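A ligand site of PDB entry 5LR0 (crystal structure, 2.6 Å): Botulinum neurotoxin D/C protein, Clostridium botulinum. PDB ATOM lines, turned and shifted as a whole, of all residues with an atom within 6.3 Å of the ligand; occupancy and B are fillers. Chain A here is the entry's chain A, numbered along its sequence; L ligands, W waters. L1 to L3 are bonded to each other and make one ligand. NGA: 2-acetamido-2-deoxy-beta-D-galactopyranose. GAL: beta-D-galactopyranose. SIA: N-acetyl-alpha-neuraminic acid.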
ATOM      1  N   ASN A 259      26.028  -0.572   4.120  1.00  0.00           N
ATOM      2  CA  ASN A 259      25.348  -1.506   3.229  1.00  0.00           C
ATOM      3  C   ASN A 259      25.412  -1.041   1.771  1.00  0.00           C
ATOM      4  O   ASN A 259      25.118   0.114   1.476  1.00  0.00           O
ATOM      5  CB  ASN A 259      23.874  -1.663   3.618  1.00  0.00           C
ATOM      6  CG  ASN A 259      23.131  -2.643   2.735  1.00  0.00           C
ATOM      7  OD1 ASN A 259      22.762  -2.327   1.596  1.00  0.00           O
ATOM      8  ND2 ASN A 259      22.890  -3.850   3.263  1.00  0.00           N
ATOM      9  N   ASN A 261      23.517  -1.223  -0.768  1.00  0.00           N
ATOM     10  CA  ASN A 261      22.345  -0.518  -1.306  1.00  0.00           C
ATOM     11  C   ASN A 261      22.202   0.921  -0.852  1.00  0.00           C
ATOM     12  O   ASN A 261      21.499   1.693  -1.489  1.00  0.00           O
ATOM     13  CB  ASN A 261      21.060  -1.269  -0.959  1.00  0.00           C
ATOM     14  CG  ASN A 261      20.803  -2.420  -1.899  1.00  0.00           C
ATOM     15  OD1 ASN A 261      21.463  -2.556  -2.913  1.00  0.00           O
ATOM     16  ND2 ASN A 261      19.813  -3.227  -1.581  1.00  0.00           N
ATOM     17  N   TYR A 262      22.893   1.285   0.229  1.00  0.00           N
ATOM     18  CA  TYR A 262      22.738   2.586   0.868  1.00  0.00           C
ATOM     19  C   TYR A 262      24.102   3.149   1.262  1.00  0.00           C
ATOM     20  O   TYR A 262      24.371   3.412   2.429  1.00  0.00           O
ATOM     21  CB  TYR A 262      21.837   2.434   2.084  1.00  0.00           C
ATOM     22  CG  TYR A 262      20.411   2.033   1.768  1.00  0.00           C
ATOM     23  CD1 TYR A 262      19.455   2.986   1.414  1.00  0.00           C
ATOM     24  CD2 TYR A 262      20.014   0.706   1.807  1.00  0.00           C
ATOM     25  CE1 TYR A 262      18.146   2.630   1.135  1.00  0.00           C
ATOM     26  CE2 TYR A 262      18.715   0.341   1.521  1.00  0.00           C
ATOM     27  CZ  TYR A 262      17.781   1.297   1.194  1.00  0.00           C
ATOM     28  OH  TYR A 262      16.491   0.932   0.907  1.00  0.00           O
ATOM     29  N   LEU A 337      11.415 -11.429  10.401  1.00  0.00           N
ATOM     30  CA  LEU A 337      12.304 -10.272  10.463  1.00  0.00           C
ATOM     31  C   LEU A 337      12.568  -9.884  11.911  1.00  0.00           C
ATOM     32  O   LEU A 337      11.633  -9.782  12.708  1.00  0.00           O
ATOM     33  CB  LEU A 337      11.697  -9.080   9.710  1.00  0.00           C
ATOM     34  CG  LEU A 337      11.501  -9.281   8.207  1.00  0.00           C
ATOM     35  CD1 LEU A 337      10.790  -8.070   7.607  1.00  0.00           C
ATOM     36  CD2 LEU A 337      12.818  -9.507   7.500  1.00  0.00           C
ATOM     37  N   SER A 386      20.345  -8.315   6.519  1.00  0.00           N
ATOM     38  CA  SER A 386      19.931  -7.477   5.391  1.00  0.00           C
ATOM     39  C   SER A 386      19.621  -6.074   5.913  1.00  0.00           C
ATOM     40  O   SER A 386      19.982  -5.730   7.033  1.00  0.00           O
ATOM     41  CB  SER A 386      18.716  -8.101   4.703  1.00  0.00           C
ATOM     42  OG  SER A 386      18.405  -7.427   3.493  1.00  0.00           O
ATOM     43  N   ILE A 387      18.912  -5.283   5.107  1.00  0.00           N
ATOM     44  CA  ILE A 387      18.585  -3.917   5.471  1.00  0.00           C
ATOM     45  C   ILE A 387      17.207  -3.565   4.918  1.00  0.00           C
ATOM     46  O   ILE A 387      16.762  -4.127   3.919  1.00  0.00           O
ATOM     47  CB  ILE A 387      19.655  -2.946   4.933  1.00  0.00           C
ATOM     48  CG1 ILE A 387      19.460  -1.530   5.484  1.00  0.00           C
ATOM     49  CG2 ILE A 387      19.663  -2.930   3.412  1.00  0.00           C
ATOM     50  CD1 ILE A 387      20.672  -0.651   5.338  1.00  0.00           C
ATOM     51  N   GLY A 388      16.505  -2.663   5.588  1.00  0.00           N
ATOM     52  CA  GLY A 388      15.227  -2.215   5.072  1.00  0.00           C
ATOM     53  C   GLY A 388      14.579  -1.089   5.832  1.00  0.00           C
ATOM     54  O   GLY A 388      14.938  -0.787   6.960  1.00  0.00           O
ATOM     55  N   SER A 389      13.592  -0.485   5.191  1.00  0.00           N
ATOM     56  CA  SER A 389      12.833   0.623   5.750  1.00  0.00           C
ATOM     57  C   SER A 389      11.569   0.089   6.380  1.00  0.00           C
ATOM     58  O   SER A 389      10.750  -0.529   5.714  1.00  0.00           O
ATOM     59  CB  SER A 389      12.511   1.596   4.638  1.00  0.00           C
ATOM     60  OG  SER A 389      11.566   2.554   5.042  1.00  0.00           O
ATOM     61  N   TYR A 390      11.437   0.314   7.698  1.00  0.00           N
ATOM     62  CA  TYR A 390      10.299  -0.178   8.459  1.00  0.00           C
ATOM     63  C   TYR A 390       9.775   0.914   9.385  1.00  0.00           C
ATOM     64  O   TYR A 390      10.541   1.752   9.866  1.00  0.00           O
ATOM     65  CB  TYR A 390      10.695  -1.423   9.258  1.00  0.00           C
ATOM     66  CG  TYR A 390      11.181  -2.522   8.366  1.00  0.00           C
ATOM     67  CD1 TYR A 390      10.270  -3.380   7.746  1.00  0.00           C
ATOM     68  CD2 TYR A 390      12.533  -2.683   8.091  1.00  0.00           C
ATOM     69  CE1 TYR A 390      10.696  -4.375   6.891  1.00  0.00           C
ATOM     70  CE2 TYR A 390      12.970  -3.685   7.245  1.00  0.00           C
ATOM     71  CZ  TYR A 390      12.051  -4.530   6.645  1.00  0.00           C
ATOM     72  OH  TYR A 390      12.468  -5.531   5.800  1.00  0.00           O
ATOM     73  N   LEU A 405      15.395   3.331   8.566  1.00  0.00           N
ATOM     74  CA  LEU A 405      16.184   2.434   7.749  1.00  0.00           C
ATOM     75  C   LEU A 405      17.149   1.696   8.676  1.00  0.00           C
ATOM     76  O   LEU A 405      18.068   2.309   9.225  1.00  0.00           O
ATOM     77  CB  LEU A 405      16.964   3.224   6.712  1.00  0.00           C
ATOM     78  CG  LEU A 405      17.750   2.406   5.707  1.00  0.00           C
ATOM     79  CD1 LEU A 405      16.815   1.648   4.767  1.00  0.00           C
ATOM     80  CD2 LEU A 405      18.682   3.308   4.922  1.00  0.00           C
ATOM     81  N   VAL A 408      18.511  -5.483   9.502  1.00  0.00           N
ATOM     82  CA  VAL A 408      17.468  -6.420   9.879  1.00  0.00           C
ATOM     83  C   VAL A 408      17.870  -7.844   9.496  1.00  0.00           C
ATOM     84  O   VAL A 408      18.449  -8.072   8.434  1.00  0.00           O
ATOM     85  CB  VAL A 408      16.117  -6.005   9.246  1.00  0.00           C
ATOM     86  CG1 VAL A 408      16.109  -6.243   7.744  1.00  0.00           C
ATOM     87  CG2 VAL A 408      14.964  -6.737   9.916  1.00  0.00           C
ATOM     88  N   LYS A 410      16.862 -11.646   8.549  1.00  0.00           N
ATOM     89  CA  LYS A 410      15.817 -12.492   7.991  1.00  0.00           C
ATOM     90  C   LYS A 410      16.103 -13.926   8.410  1.00  0.00           C
ATOM     91  O   LYS A 410      17.052 -14.541   7.915  1.00  0.00           O
ATOM     92  CB  LYS A 410      15.831 -12.376   6.465  1.00  0.00           C
ATOM     93  CG  LYS A 410      14.902 -13.320   5.725  1.00  0.00           C
ATOM     94  CD  LYS A 410      13.452 -12.855   5.716  1.00  0.00           C
ATOM     95  CE  LYS A 410      12.822 -13.122   4.358  1.00  0.00           C
ATOM     96  NZ  LYS A 410      11.352 -13.257   4.446  1.00  0.00           N
ATOM     97  N   LEU A 417      17.061 -13.998  -0.432  1.00  0.00           N
ATOM     98  CA  LEU A 417      18.014 -12.926  -0.152  1.00  0.00           C
ATOM     99  C   LEU A 417      19.479 -13.273  -0.390  1.00  0.00           C
ATOM    100  O   LEU A 417      20.325 -12.382  -0.376  1.00  0.00           O
ATOM    101  CB  LEU A 417      17.852 -12.419   1.276  1.00  0.00           C
ATOM    102  CG  LEU A 417      16.575 -11.661   1.607  1.00  0.00           C
ATOM    103  CD1 LEU A 417      16.609 -11.265   3.071  1.00  0.00           C
ATOM    104  CD2 LEU A 417      16.381 -10.434   0.725  1.00  0.00           C
ATOM    105  N   SER A 420      20.675 -11.386  -3.111  1.00  0.00           N
ATOM    106  CA  SER A 420      20.267  -9.986  -2.976  1.00  0.00           C
ATOM    107  C   SER A 420      21.418  -9.130  -2.489  1.00  0.00           C
ATOM    108  O   SER A 420      22.147  -9.481  -1.563  1.00  0.00           O
ATOM    109  CB  SER A 420      19.078  -9.844  -2.028  1.00  0.00           C
ATOM    110  OG  SER A 420      18.776  -8.480  -1.826  1.00  0.00           O
ATOM    111  N   SER A 422      21.262  -6.381  -0.972  1.00  0.00           N
ATOM    112  CA  SER A 422      20.971  -5.837   0.355  1.00  0.00           C
ATOM    113  C   SER A 422      21.653  -6.599   1.498  1.00  0.00           C
ATOM    114  O   SER A 422      21.611  -6.150   2.649  1.00  0.00           O
ATOM    115  CB  SER A 422      19.463  -5.860   0.607  1.00  0.00           C
ATOM    116  OG  SER A 422      18.992  -7.181   0.812  1.00  0.00           O
ATOM    117  N   THR A 423      22.252  -7.751   1.196  1.00  0.00           N
ATOM    118  CA  THR A 423      22.989  -8.524   2.183  1.00  0.00           C
ATOM    119  C   THR A 423      24.506  -8.352   2.032  1.00  0.00           C
ATOM    120  O   THR A 423      25.275  -9.056   2.664  1.00  0.00           O
ATOM    121  CB  THR A 423      22.637 -10.019   2.067  1.00  0.00           C
ATOM    122  OG1 THR A 423      23.088 -10.516   0.802  1.00  0.00           O
ATOM    123  CG2 THR A 423      21.142 -10.225   2.157  1.00  0.00           C
HETATM  124  C1  NGA L   1       8.028   0.495  -5.110  1.00  0.00           C
HETATM  125  C2  NGA L   1       8.940  -0.693  -5.063  1.00  0.00           C
HETATM  126  C3  NGA L   1      10.194  -0.165  -4.419  1.00  0.00           C
HETATM  127  C4  NGA L   1      10.830   0.914  -5.263  1.00  0.00           C
HETATM  128  C5  NGA L   1       9.797   1.999  -5.350  1.00  0.00           C
HETATM  129  C6  NGA L   1      10.270   3.114  -6.233  1.00  0.00           C
HETATM  130  C7  NGA L   1       8.425  -3.011  -4.729  1.00  0.00           C
HETATM  131  C8  NGA L   1       8.037  -4.087  -3.812  1.00  0.00           C
HETATM  132  N2  NGA L   1       8.396  -1.776  -4.301  1.00  0.00           N
HETATM  133  O1  NGA L   1       7.002   0.149  -5.920  1.00  0.00           O
HETATM  134  O3  NGA L   1      11.104  -1.188  -4.186  1.00  0.00           O
HETATM  135  O4  NGA L   1      10.989   0.526  -6.597  1.00  0.00           O
HETATM  136  O5  NGA L   1       8.648   1.450  -5.929  1.00  0.00           O
HETATM  137  O6  NGA L   1       9.112   3.699  -6.758  1.00  0.00           O
HETATM  138  O7  NGA L   1       8.766  -3.283  -5.822  1.00  0.00           O
HETATM  139  C1  GAL L   2      11.809  -0.831  -3.061  1.00  0.00           C
HETATM  140  C2  GAL L   2      12.738  -1.983  -2.857  1.00  0.00           C
HETATM  141  C3  GAL L   2      13.758  -1.658  -1.782  1.00  0.00           C
HETATM  142  C4  GAL L   2      14.378  -0.278  -1.941  1.00  0.00           C
HETATM  143  C5  GAL L   2      13.303   0.740  -2.207  1.00  0.00           C
HETATM  144  C6  GAL L   2      13.891   2.069  -2.571  1.00  0.00           C
HETATM  145  O2  GAL L   2      11.939  -3.065  -2.458  1.00  0.00           O
HETATM  146  O3  GAL L   2      14.759  -2.642  -1.890  1.00  0.00           O
HETATM  147  O4  GAL L   2      15.318  -0.252  -2.979  1.00  0.00           O
HETATM  148  O5  GAL L   2      12.613   0.271  -3.313  1.00  0.00           O
HETATM  149  O6  GAL L   2      13.026   3.085  -2.107  1.00  0.00           O
HETATM  150  C1  SIA L   3      16.126  -2.468   0.085  1.00  0.00           C
HETATM  151  C2  SIA L   3      15.198  -3.366  -0.685  1.00  0.00           C
HETATM  152  C3  SIA L   3      15.863  -4.779  -0.744  1.00  0.00           C
HETATM  153  C4  SIA L   3      15.971  -5.476   0.557  1.00  0.00           C
HETATM  154  C5  SIA L   3      14.728  -5.467   1.354  1.00  0.00           C
HETATM  155  C6  SIA L   3      14.186  -4.069   1.446  1.00  0.00           C
HETATM  156  C7  SIA L   3      12.867  -4.086   2.204  1.00  0.00           C
HETATM  157  C8  SIA L   3      12.233  -2.718   2.304  1.00  0.00           C
HETATM  158  C9  SIA L   3      11.238  -2.638   3.430  1.00  0.00           C
HETATM  159  C10 SIA L   3      14.698  -7.117   3.147  1.00  0.00           C
HETATM  160  C11 SIA L   3      15.105  -7.360   4.528  1.00  0.00           C
HETATM  161  N5  SIA L   3      15.079  -5.970   2.644  1.00  0.00           N
HETATM  162  O1A SIA L   3      15.696  -1.790   1.012  1.00  0.00           O
HETATM  163  O1B SIA L   3      17.312  -2.386  -0.209  1.00  0.00           O
HETATM  164  O4  SIA L   3      16.171  -6.812   0.209  1.00  0.00           O
HETATM  165  O6  SIA L   3      14.056  -3.532   0.133  1.00  0.00           O
HETATM  166  O7  SIA L   3      11.964  -4.966   1.580  1.00  0.00           O
HETATM  167  O8  SIA L   3      13.248  -1.811   2.601  1.00  0.00           O
HETATM  168  O9  SIA L   3      10.587  -1.388   3.438  1.00  0.00           O
HETATM  169  O10 SIA L   3      14.085  -7.911   2.555  1.00  0.00           O
HETATM  170  O   HOH W   1      11.184  -6.494   3.981  1.00  0.00           O
HETATM  171  O   HOH W   2       7.799  -2.015  -1.736  1.00  0.00           O
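The side-chain hydroxyl of Ser 422 is in hydrogen-bond range of an oxygen (O4) of SIA L3, 2.9 Å away.
The backbone carbonyl oxygen (O) of Ile 387 sits at hydrogen-bond distance from a nitrogen (N5) of SIA L3.
O9 of SIA L3 is in hydrogen-bond range of O of Ser 389, at 2.4 Å.
The side-chain hydroxyl of Tyr 262 sits at hydrogen-bond distance from an oxygen (O1A) of SIA L3 (2.8 Å).
An oxygen (O8) of SIA L3 is in hydrogen-bond range of the backbone NH of Ser 389, 2.9 Å away.
ND2 of Asn 261 is in hydrogen-bond range of O1B of SIA L3 (3.0 Å).
Merely in contact with the ligand: Ser 386, Gly 388, Tyr 390, Val 408, Leu 417 and Ser 420.
Hydrophobic or aromatic side chains within 4 Å of the ligand: Tyr 262, Tyr 390, Val 408 and Leu 417.
The nearest printed residue that does not touch the ligand is Leu 337 (4.3 Å).
Water W1 bridges OH of Tyr 390 (2.4 Å) and O7 of SIA L3 (3.0 Å).
The backbone carbonyl oxygen (O) of Ser 420 sits at hydrogen-bond distance from the side-chain hydroxyl (OG1) of Thr 423, at 2.7 Å.
OG of Ser 422 sits at hydrogen-bond distance from OG of Ser 386 (2.8 Å).
O of Val 408 is in hydrogen-bond range of N of Ser 386 (2.7 Å).
ND2 of Asn 259 is in hydrogen-bond range of O of Ser 422, 2.7 Å away.
The side-chain hydroxyl (OG) of Ser 422 lies within hydrogen-bond range of the side-chain hydroxyl (OG) of Ser 420 (2.9 Å).
N of Asn 261 is in hydrogen-bond range of OD1 of Asn 259 (2.7 Å).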
